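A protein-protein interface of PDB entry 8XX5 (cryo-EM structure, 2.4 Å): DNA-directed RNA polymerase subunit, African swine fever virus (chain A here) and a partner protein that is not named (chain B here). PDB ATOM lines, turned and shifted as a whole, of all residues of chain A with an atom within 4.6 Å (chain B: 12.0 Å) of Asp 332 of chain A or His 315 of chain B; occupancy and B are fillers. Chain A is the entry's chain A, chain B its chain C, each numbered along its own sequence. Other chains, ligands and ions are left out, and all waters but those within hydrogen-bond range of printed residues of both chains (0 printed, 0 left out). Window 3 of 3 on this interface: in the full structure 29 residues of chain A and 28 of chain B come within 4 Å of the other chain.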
ATOM      1  N   ASN A 330       3.157  27.844   4.863  1.00  0.00           N
ATOM      2  CA  ASN A 330       1.845  27.547   5.432  1.00  0.00           C
ATOM      3  C   ASN A 330       1.699  26.029   5.421  1.00  0.00           C
ATOM      4  O   ASN A 330       1.397  25.440   4.381  1.00  0.00           O
ATOM      5  CB  ASN A 330       0.732  28.228   4.648  1.00  0.00           C
ATOM      6  CG  ASN A 330      -0.600  28.196   5.374  1.00  0.00           C
ATOM      7  OD1 ASN A 330      -0.872  27.296   6.164  1.00  0.00           O
ATOM      8  ND2 ASN A 330      -1.441  29.184   5.103  1.00  0.00           N
ATOM      9  N   SER A 331       1.918  25.408   6.580  1.00  0.00           N
ATOM     10  CA  SER A 331       1.864  23.955   6.673  1.00  0.00           C
ATOM     11  C   SER A 331       0.443  23.411   6.623  1.00  0.00           C
ATOM     12  O   SER A 331       0.271  22.194   6.505  1.00  0.00           O
ATOM     13  CB  SER A 331       2.556  23.487   7.955  1.00  0.00           C
ATOM     14  OG  SER A 331       1.916  24.010   9.104  1.00  0.00           O
ATOM     15  N   ASP A 332      -0.569  24.269   6.702  1.00  0.00           N
ATOM     16  CA  ASP A 332      -1.958  23.843   6.610  1.00  0.00           C
ATOM     17  C   ASP A 332      -2.471  23.801   5.178  1.00  0.00           C
ATOM     18  O   ASP A 332      -3.641  23.473   4.963  1.00  0.00           O
ATOM     19  CB  ASP A 332      -2.848  24.761   7.449  1.00  0.00           C
ATOM     20  CG  ASP A 332      -2.855  24.379   8.912  1.00  0.00           C
ATOM     21  OD1 ASP A 332      -2.913  23.168   9.211  1.00  0.00           O
ATOM     22  OD2 ASP A 332      -2.799  25.288   9.765  1.00  0.00           O
ATOM     23  N   LEU A 333      -1.633  24.126   4.202  1.00  0.00           N
ATOM     24  CA  LEU A 333      -1.988  24.037   2.796  1.00  0.00           C
ATOM     25  C   LEU A 333      -1.439  22.745   2.212  1.00  0.00           C
ATOM     26  O   LEU A 333      -0.349  22.300   2.579  1.00  0.00           O
ATOM     27  CB  LEU A 333      -1.441  25.229   2.010  1.00  0.00           C
ATOM     28  CG  LEU A 333      -1.975  26.621   2.348  1.00  0.00           C
ATOM     29  CD1 LEU A 333      -1.204  27.671   1.573  1.00  0.00           C
ATOM     30  CD2 LEU A 333      -3.458  26.718   2.056  1.00  0.00           C
ATOM     31  N   HIS A 334      -2.201  22.144   1.305  1.00  0.00           N
ATOM     32  CA  HIS A 334      -1.720  20.976   0.589  1.00  0.00           C
ATOM     33  C   HIS A 334      -0.600  21.371  -0.369  1.00  0.00           C
ATOM     34  O   HIS A 334      -0.402  22.545  -0.689  1.00  0.00           O
ATOM     35  CB  HIS A 334      -2.861  20.307  -0.173  1.00  0.00           C
ATOM     36  CG  HIS A 334      -3.843  19.603   0.708  1.00  0.00           C
ATOM     37  ND1 HIS A 334      -4.856  20.264   1.368  1.00  0.00           N
ATOM     38  CD2 HIS A 334      -3.966  18.298   1.041  1.00  0.00           C
ATOM     39  CE1 HIS A 334      -5.563  19.395   2.068  1.00  0.00           C
ATOM     40  NE2 HIS A 334      -5.043  18.195   1.888  1.00  0.00           N
ATOM     41  N   VAL A 434      -6.291  28.771  -2.627  1.00  0.00           N
ATOM     42  CA  VAL A 434      -6.954  28.902  -1.337  1.00  0.00           C
ATOM     43  C   VAL A 434      -6.932  30.384  -1.000  1.00  0.00           C
ATOM     44  O   VAL A 434      -5.865  30.950  -0.733  1.00  0.00           O
ATOM     45  CB  VAL A 434      -6.272  28.070  -0.243  1.00  0.00           C
ATOM     46  CG1 VAL A 434      -6.899  28.360   1.107  1.00  0.00           C
ATOM     47  CG2 VAL A 434      -6.360  26.590  -0.571  1.00  0.00           C
ATOM     48  N   LEU A 436      -7.119  33.537   1.075  1.00  0.00           N
ATOM     49  CA  LEU A 436      -6.939  33.917   2.469  1.00  0.00           C
ATOM     50  C   LEU A 436      -7.759  35.174   2.728  1.00  0.00           C
ATOM     51  O   LEU A 436      -7.455  36.244   2.193  1.00  0.00           O
ATOM     52  CB  LEU A 436      -5.461  34.134   2.776  1.00  0.00           C
ATOM     53  CG  LEU A 436      -4.556  33.024   2.239  1.00  0.00           C
ATOM     54  CD1 LEU A 436      -3.110  33.472   2.196  1.00  0.00           C
ATOM     55  CD2 LEU A 436      -4.706  31.761   3.067  1.00  0.00           C
ATOM     56  N   THR A 533      -5.248  17.461  11.841  1.00  0.00           N
ATOM     57  CA  THR A 533      -4.980  18.344  10.714  1.00  0.00           C
ATOM     58  C   THR A 533      -4.591  17.593   9.446  1.00  0.00           C
ATOM     59  O   THR A 533      -4.191  18.226   8.464  1.00  0.00           O
ATOM     60  CB  THR A 533      -3.884  19.348  11.081  1.00  0.00           C
ATOM     61  OG1 THR A 533      -2.599  18.740  10.914  1.00  0.00           O
ATOM     62  CG2 THR A 533      -4.037  19.801  12.524  1.00  0.00           C
ATOM     63  N   GLN A 535      -6.386  16.299   7.256  1.00  0.00           N
ATOM     64  CA  GLN A 535      -7.324  16.608   6.180  1.00  0.00           C
ATOM     65  C   GLN A 535      -7.849  15.349   5.499  1.00  0.00           C
ATOM     66  O   GLN A 535      -8.573  15.433   4.502  1.00  0.00           O
ATOM     67  CB  GLN A 535      -6.682  17.540   5.150  1.00  0.00           C
ATOM     68  CG  GLN A 535      -7.347  18.898   5.051  1.00  0.00           C
ATOM     69  CD  GLN A 535      -6.900  19.843   6.143  1.00  0.00           C
ATOM     70  OE1 GLN A 535      -7.331  19.732   7.289  1.00  0.00           O
ATOM     71  NE2 GLN A 535      -6.034  20.785   5.792  1.00  0.00           N
ATOM     72  N   PHE A 634       1.433  15.383   2.530  1.00  0.00           N
ATOM     73  CA  PHE A 634       0.757  16.309   3.432  1.00  0.00           C
ATOM     74  C   PHE A 634       0.306  15.610   4.709  1.00  0.00           C
ATOM     75  O   PHE A 634       0.478  16.143   5.811  1.00  0.00           O
ATOM     76  CB  PHE A 634      -0.435  16.964   2.738  1.00  0.00           C
ATOM     77  CG  PHE A 634      -1.190  17.923   3.617  1.00  0.00           C
ATOM     78  CD1 PHE A 634      -0.719  19.205   3.829  1.00  0.00           C
ATOM     79  CD2 PHE A 634      -2.360  17.535   4.246  1.00  0.00           C
ATOM     80  CE1 PHE A 634      -1.402  20.084   4.643  1.00  0.00           C
ATOM     81  CE2 PHE A 634      -3.046  18.409   5.061  1.00  0.00           C
ATOM     82  CZ  PHE A 634      -2.567  19.686   5.258  1.00  0.00           C
ATOM     83  N   GLN A 638       1.664  16.415   8.464  1.00  0.00           N
ATOM     84  CA  GLN A 638       0.778  16.797   9.558  1.00  0.00           C
ATOM     85  C   GLN A 638       0.966  15.885  10.761  1.00  0.00           C
ATOM     86  O   GLN A 638       0.976  16.351  11.904  1.00  0.00           O
ATOM     87  CB  GLN A 638      -0.678  16.773   9.094  1.00  0.00           C
ATOM     88  CG  GLN A 638      -1.005  17.790   8.023  1.00  0.00           C
ATOM     89  CD  GLN A 638      -0.376  19.137   8.291  1.00  0.00           C
ATOM     90  OE1 GLN A 638       0.486  19.590   7.539  1.00  0.00           O
ATOM     91  NE2 GLN A 638      -0.803  19.786   9.364  1.00  0.00           N
ATOM     92  N   ARG B 171      -7.393  39.091  21.637  1.00  0.00           N
ATOM     93  CA  ARG B 171      -7.033  38.390  20.410  1.00  0.00           C
ATOM     94  C   ARG B 171      -7.243  39.243  19.165  1.00  0.00           C
ATOM     95  O   ARG B 171      -6.699  38.912  18.107  1.00  0.00           O
ATOM     96  CB  ARG B 171      -7.826  37.088  20.290  1.00  0.00           C
ATOM     97  CG  ARG B 171      -9.239  37.165  20.823  1.00  0.00           C
ATOM     98  CD  ARG B 171      -9.985  35.869  20.571  1.00  0.00           C
ATOM     99  NE  ARG B 171      -9.861  35.430  19.187  1.00  0.00           N
ATOM    100  CZ  ARG B 171     -10.865  35.385  18.323  1.00  0.00           C
ATOM    101  NH1 ARG B 171     -12.090  35.747  18.668  1.00  0.00           N
ATOM    102  NH2 ARG B 171     -10.636  34.965  17.083  1.00  0.00           N
ATOM    103  N   THR B 282     -18.678  23.578  12.870  1.00  0.00           N
ATOM    104  CA  THR B 282     -17.821  24.654  12.387  1.00  0.00           C
ATOM    105  C   THR B 282     -18.297  25.964  12.999  1.00  0.00           C
ATOM    106  O   THR B 282     -19.413  26.415  12.724  1.00  0.00           O
ATOM    107  CB  THR B 282     -17.840  24.728  10.861  1.00  0.00           C
ATOM    108  OG1 THR B 282     -17.610  23.426  10.314  1.00  0.00           O
ATOM    109  CG2 THR B 282     -16.768  25.682  10.362  1.00  0.00           C
ATOM    110  N   ILE B 283     -17.454  26.571  13.829  1.00  0.00           N
ATOM    111  CA  ILE B 283     -17.751  27.847  14.466  1.00  0.00           C
ATOM    112  C   ILE B 283     -16.742  28.868  13.965  1.00  0.00           C
ATOM    113  O   ILE B 283     -15.528  28.677  14.114  1.00  0.00           O
ATOM    114  CB  ILE B 283     -17.709  27.743  15.997  1.00  0.00           C
ATOM    115  CG1 ILE B 283     -18.610  26.602  16.477  1.00  0.00           C
ATOM    116  CG2 ILE B 283     -18.113  29.067  16.625  1.00  0.00           C
ATOM    117  CD1 ILE B 283     -20.002  27.033  16.868  1.00  0.00           C
ATOM    118  N   LYS B 284     -17.236  29.954  13.379  1.00  0.00           N
ATOM    119  CA  LYS B 284     -16.364  31.013  12.897  1.00  0.00           C
ATOM    120  C   LYS B 284     -15.867  31.865  14.057  1.00  0.00           C
ATOM    121  O   LYS B 284     -16.602  32.128  15.015  1.00  0.00           O
ATOM    122  CB  LYS B 284     -17.093  31.889  11.879  1.00  0.00           C
ATOM    123  CG  LYS B 284     -17.112  31.311  10.476  1.00  0.00           C
ATOM    124  CD  LYS B 284     -16.596  32.316   9.461  1.00  0.00           C
ATOM    125  CE  LYS B 284     -15.094  32.176   9.257  1.00  0.00           C
ATOM    126  NZ  LYS B 284     -14.756  31.019   8.385  1.00  0.00           N
ATOM    127  N   ASP B 285     -14.607  32.294  13.962  1.00  0.00           N
ATOM    128  CA  ASP B 285     -13.962  33.134  14.973  1.00  0.00           C
ATOM    129  C   ASP B 285     -13.939  32.468  16.345  1.00  0.00           C
ATOM    130  O   ASP B 285     -14.031  33.139  17.375  1.00  0.00           O
ATOM    131  CB  ASP B 285     -14.624  34.512  15.060  1.00  0.00           C
ATOM    132  CG  ASP B 285     -13.626  35.622  15.327  1.00  0.00           C
ATOM    133  OD1 ASP B 285     -12.576  35.653  14.653  1.00  0.00           O
ATOM    134  OD2 ASP B 285     -13.892  36.463  16.211  1.00  0.00           O
ATOM    135  N   GLU B 286     -13.811  31.146  16.370  1.00  0.00           N
ATOM    136  CA  GLU B 286     -13.660  30.390  17.604  1.00  0.00           C
ATOM    137  C   GLU B 286     -12.212  29.944  17.748  1.00  0.00           C
ATOM    138  O   GLU B 286     -11.569  29.562  16.766  1.00  0.00           O
ATOM    139  CB  GLU B 286     -14.592  29.179  17.631  1.00  0.00           C
ATOM    140  CG  GLU B 286     -14.990  28.745  19.028  1.00  0.00           C
ATOM    141  CD  GLU B 286     -15.742  29.822  19.780  1.00  0.00           C
ATOM    142  OE1 GLU B 286     -16.952  29.988  19.527  1.00  0.00           O
ATOM    143  OE2 GLU B 286     -15.124  30.502  20.625  1.00  0.00           O
ATOM    144  N   THR B 287     -11.706  29.994  18.974  1.00  0.00           N
ATOM    145  CA  THR B 287     -10.295  29.789  19.248  1.00  0.00           C
ATOM    146  C   THR B 287     -10.044  28.367  19.744  1.00  0.00           C
ATOM    147  O   THR B 287     -10.929  27.508  19.731  1.00  0.00           O
ATOM    148  CB  THR B 287      -9.808  30.828  20.259  1.00  0.00           C
ATOM    149  OG1 THR B 287     -10.229  30.450  21.574  1.00  0.00           O
ATOM    150  CG2 THR B 287     -10.380  32.193  19.928  1.00  0.00           C
ATOM    151  N   HIS B 288      -8.808  28.112  20.180  1.00  0.00           N
ATOM    152  CA  HIS B 288      -8.446  26.804  20.707  1.00  0.00           C
ATOM    153  C   HIS B 288      -9.073  26.527  22.064  1.00  0.00           C
ATOM    154  O   HIS B 288      -9.149  25.363  22.464  1.00  0.00           O
ATOM    155  CB  HIS B 288      -6.927  26.681  20.817  1.00  0.00           C
ATOM    156  CG  HIS B 288      -6.234  26.562  19.498  1.00  0.00           C
ATOM    157  ND1 HIS B 288      -5.987  25.347  18.896  1.00  0.00           N
ATOM    158  CD2 HIS B 288      -5.733  27.503  18.666  1.00  0.00           C
ATOM    159  CE1 HIS B 288      -5.365  25.546  17.749  1.00  0.00           C
ATOM    160  NE2 HIS B 288      -5.198  26.845  17.585  1.00  0.00           N
ATOM    161  N   TYR B 310     -10.354  18.575  16.663  1.00  0.00           N
ATOM    162  CA  TYR B 310     -10.676  19.903  16.169  1.00  0.00           C
ATOM    163  C   TYR B 310      -9.455  20.493  15.483  1.00  0.00           C
ATOM    164  O   TYR B 310      -8.321  20.067  15.712  1.00  0.00           O
ATOM    165  CB  TYR B 310     -11.154  20.824  17.298  1.00  0.00           C
ATOM    166  CG  TYR B 310     -10.041  21.380  18.154  1.00  0.00           C
ATOM    167  CD1 TYR B 310      -9.432  20.599  19.125  1.00  0.00           C
ATOM    168  CD2 TYR B 310      -9.604  22.685  17.995  1.00  0.00           C
ATOM    169  CE1 TYR B 310      -8.418  21.103  19.909  1.00  0.00           C
ATOM    170  CE2 TYR B 310      -8.591  23.197  18.774  1.00  0.00           C
ATOM    171  CZ  TYR B 310      -8.001  22.403  19.730  1.00  0.00           C
ATOM    172  OH  TYR B 310      -6.990  22.914  20.508  1.00  0.00           O
ATOM    173  N   GLN B 311      -9.701  21.483  14.630  1.00  0.00           N
ATOM    174  CA  GLN B 311      -8.630  22.209  13.960  1.00  0.00           C
ATOM    175  C   GLN B 311      -8.983  23.686  13.931  1.00  0.00           C
ATOM    176  O   GLN B 311      -9.982  24.075  13.319  1.00  0.00           O
ATOM    177  CB  GLN B 311      -8.401  21.680  12.540  1.00  0.00           C
ATOM    178  CG  GLN B 311      -9.671  21.315  11.796  1.00  0.00           C
ATOM    179  CD  GLN B 311      -9.408  20.418  10.605  1.00  0.00           C
ATOM    180  OE1 GLN B 311     -10.270  19.640  10.196  1.00  0.00           O
ATOM    181  NE2 GLN B 311      -8.210  20.521  10.041  1.00  0.00           N
ATOM    182  N   CYS B 312      -8.177  24.503  14.607  1.00  0.00           N
ATOM    183  CA  CYS B 312      -8.265  25.958  14.494  1.00  0.00           C
ATOM    184  C   CYS B 312      -7.154  26.416  13.556  1.00  0.00           C
ATOM    185  O   CYS B 312      -6.130  26.955  13.975  1.00  0.00           O
ATOM    186  CB  CYS B 312      -8.160  26.623  15.862  1.00  0.00           C
ATOM    187  SG  CYS B 312      -9.405  26.110  17.049  1.00  0.00           S
ATOM    188  N   VAL B 313      -7.369  26.189  12.266  1.00  0.00           N
ATOM    189  CA  VAL B 313      -6.373  26.602  11.269  1.00  0.00           C
ATOM    190  C   VAL B 313      -6.215  28.117  11.326  1.00  0.00           C
ATOM    191  O   VAL B 313      -7.229  28.841  11.360  1.00  0.00           O
ATOM    192  CB  VAL B 313      -6.793  26.141   9.864  1.00  0.00           C
ATOM    193  CG1 VAL B 313      -5.754  26.542   8.842  1.00  0.00           C
ATOM    194  CG2 VAL B 313      -7.001  24.636   9.844  1.00  0.00           C
ATOM    195  N   PRO B 314      -4.989  28.645  11.381  1.00  0.00           N
ATOM    196  CA  PRO B 314      -4.829  30.105  11.503  1.00  0.00           C
ATOM    197  C   PRO B 314      -5.512  30.882  10.393  1.00  0.00           C
ATOM    198  O   PRO B 314      -6.098  31.939  10.654  1.00  0.00           O
ATOM    199  CB  PRO B 314      -3.307  30.286  11.481  1.00  0.00           C
ATOM    200  CG  PRO B 314      -2.773  28.995  12.000  1.00  0.00           C
ATOM    201  CD  PRO B 314      -3.702  27.936  11.489  1.00  0.00           C
ATOM    202  N   HIS B 315      -5.458  30.391   9.160  1.00  0.00           N
ATOM    203  CA  HIS B 315      -6.321  30.919   8.120  1.00  0.00           C
ATOM    204  C   HIS B 315      -7.633  30.138   8.112  1.00  0.00           C
ATOM    205  O   HIS B 315      -7.737  29.048   8.676  1.00  0.00           O
ATOM    206  CB  HIS B 315      -5.628  30.880   6.756  1.00  0.00           C
ATOM    207  CG  HIS B 315      -5.586  29.524   6.125  1.00  0.00           C
ATOM    208  ND1 HIS B 315      -4.584  28.614   6.381  1.00  0.00           N
ATOM    209  CD2 HIS B 315      -6.415  28.930   5.235  1.00  0.00           C
ATOM    210  CE1 HIS B 315      -4.802  27.515   5.681  1.00  0.00           C
ATOM    211  NE2 HIS B 315      -5.907  27.681   4.979  1.00  0.00           N
ATOM    212  N   LYS B 316      -8.644  30.720   7.472  1.00  0.00           N
ATOM    213  CA  LYS B 316     -10.054  30.343   7.483  1.00  0.00           C
ATOM    214  C   LYS B 316     -10.736  30.765   8.784  1.00  0.00           C
ATOM    215  O   LYS B 316     -11.965  30.729   8.848  1.00  0.00           O
ATOM    216  CB  LYS B 316     -10.291  28.834   7.270  1.00  0.00           C
ATOM    217  CG  LYS B 316     -10.178  28.368   5.831  1.00  0.00           C
ATOM    218  CD  LYS B 316     -10.407  26.870   5.733  1.00  0.00           C
ATOM    219  CE  LYS B 316      -9.275  26.100   6.394  1.00  0.00           C
ATOM    220  NZ  LYS B 316      -9.455  24.626   6.283  1.00  0.00           N
ATOM    221  N   GLN B 317      -9.987  31.196   9.797  1.00  0.00           N
ATOM    222  CA  GLN B 317     -10.498  31.824  11.019  1.00  0.00           C
ATOM    223  C   GLN B 317     -11.764  31.145  11.547  1.00  0.00           C
ATOM    224  O   GLN B 317     -12.814  31.764  11.717  1.00  0.00           O
ATOM    225  CB  GLN B 317     -10.739  33.315  10.786  1.00  0.00           C
ATOM    226  CG  GLN B 317      -9.596  34.015  10.064  1.00  0.00           C
ATOM    227  CD  GLN B 317     -10.076  34.909   8.937  1.00  0.00           C
ATOM    228  OE1 GLN B 317     -10.324  36.098   9.135  1.00  0.00           O
ATOM    229  NE2 GLN B 317     -10.207  34.340   7.744  1.00  0.00           N
ATOM    230  N   GLU B 318     -11.647  29.847  11.817  1.00  0.00           N
ATOM    231  CA  GLU B 318     -12.785  29.100  12.335  1.00  0.00           C
ATOM    232  C   GLU B 318     -12.293  27.863  13.069  1.00  0.00           C
ATOM    233  O   GLU B 318     -11.161  27.411  12.880  1.00  0.00           O
ATOM    234  CB  GLU B 318     -13.754  28.707  11.213  1.00  0.00           C
ATOM    235  CG  GLU B 318     -13.392  27.418  10.503  1.00  0.00           C
ATOM    236  CD  GLU B 318     -13.669  27.477   9.016  1.00  0.00           C
ATOM    237  OE1 GLU B 318     -13.288  26.528   8.300  1.00  0.00           O
ATOM    238  OE2 GLU B 318     -14.269  28.473   8.561  1.00  0.00           O
ATOM    239  N   MET B 319     -13.168  27.322  13.913  1.00  0.00           N
ATOM    240  CA  MET B 319     -12.929  26.076  14.628  1.00  0.00           C
ATOM    241  C   MET B 319     -13.837  24.999  14.055  1.00  0.00           C
ATOM    242  O   MET B 319     -15.054  25.187  13.974  1.00  0.00           O
ATOM    243  CB  MET B 319     -13.187  26.244  16.128  1.00  0.00           C
ATOM    244  CG  MET B 319     -12.720  25.076  16.989  1.00  0.00           C
ATOM    245  SD  MET B 319     -13.943  23.768  17.187  1.00  0.00           S
ATOM    246  CE  MET B 319     -15.271  24.659  17.989  1.00  0.00           C
ATOM    247  N   VAL B 320     -13.247  23.874  13.663  1.00  0.00           N
ATOM    248  CA  VAL B 320     -13.981  22.762  13.073  1.00  0.00           C
ATOM    249  C   VAL B 320     -13.774  21.547  13.965  1.00  0.00           C
ATOM    250  O   VAL B 320     -12.692  20.948  13.968  1.00  0.00           O
ATOM    251  CB  VAL B 320     -13.532  22.472  11.636  1.00  0.00           C
ATOM    252  CG1 VAL B 320     -14.323  21.315  11.060  1.00  0.00           C
ATOM    253  CG2 VAL B 320     -13.694  23.710  10.775  1.00  0.00           C
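The side-chain amide nitrogen (NE2) of Gln 311 of chain B is in hydrogen-bond range of the side-chain amide oxygen (OE1) of Gln 535 of chain A (3.0 Å).
ND2 of Asn 330 of chain A sits at hydrogen-bond distance from ND1 of His 315 of chain B (3.4 Å).
N of Gln 311 of chain B is in hydrogen-bond range of O of Val 320 of chain B (3.1 Å).
OD1 of Asn 330 of chain A lies within hydrogen-bond range of N of Asp 332 of chain A, 3.1 Å away.
OG1 of Thr 533 of chain A is in hydrogen-bond range of NE2 of Gln 638 of chain A.
Among the printed residues, merely in contact across the chains: Asp 332 of chain A with Pro 314 of chain B (3.3 Å), Asp 332 of chain A with Val 313 of chain B (3.3 Å), Asp 332 of chain A with His 315 of chain B (3.8 Å), Leu 436 of chain A with His 315 of chain B (3.9 Å), Leu 333 of chain A with His 315 of chain B (3.9 Å) and Thr 533 of chain A with Gln 311 of chain B (3.95 Å).
Of chain B, only His 315 (3.4 Å) comes within 4 Å of Asn 330 of chain A.
No residue of chain B comes within 4 Å of Ser 331 of chain A.
Asp 332 of chain A touches three residues of chain B.
Of chain B, only His 315 comes within 4 Å of Leu 333 of chain A.
No residue of chain B comes within 4 Å of His 334 of chain A.
Val 434 of chain A touches none of the printed residues of chain B.
Thr 533 of chain A touches just one residue of chain B: Gln 311 (3.95 Å).
Of the printed residues of chain B, Gln 535 of chain A touches Gln 311.
Of the printed residues of chain A, Gln 311 of chain B touches Thr 533 (3.95 Å) and Gln 535 (3.0 Å).
Of the printed residues of chain A, Val 313 of chain B touches Asp 332.
Printed residues of chain A within 4 Å of Pro 314 of chain B: Asp 332.
His 315 of chain B touches four residues of chain A.
Gln 317 of chain B touches none of the printed residues of chain A.
The nearest residue of chain B that does not touch Asp 332 of chain A is Cys 312 of chain B (5.6 Å).
The nearest residue of chain A that does not touch His 315 of chain B is Val 434 of chain A (4.1 Å).
Of the 11 printed residues of chain A, 6 touch a printed residue of chain B.
Hydrophobic or aromatic side chains of chain A within 4 Å of the printed part of chain B: Leu 333 and Leu 436.
Printed residues of chain B that touch a printed residue of chain A: Gln 311, Val 313, Pro 314 and His 315.
Along chain B the printed residues that touch a printed residue of chain A span positions 311 to 315.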
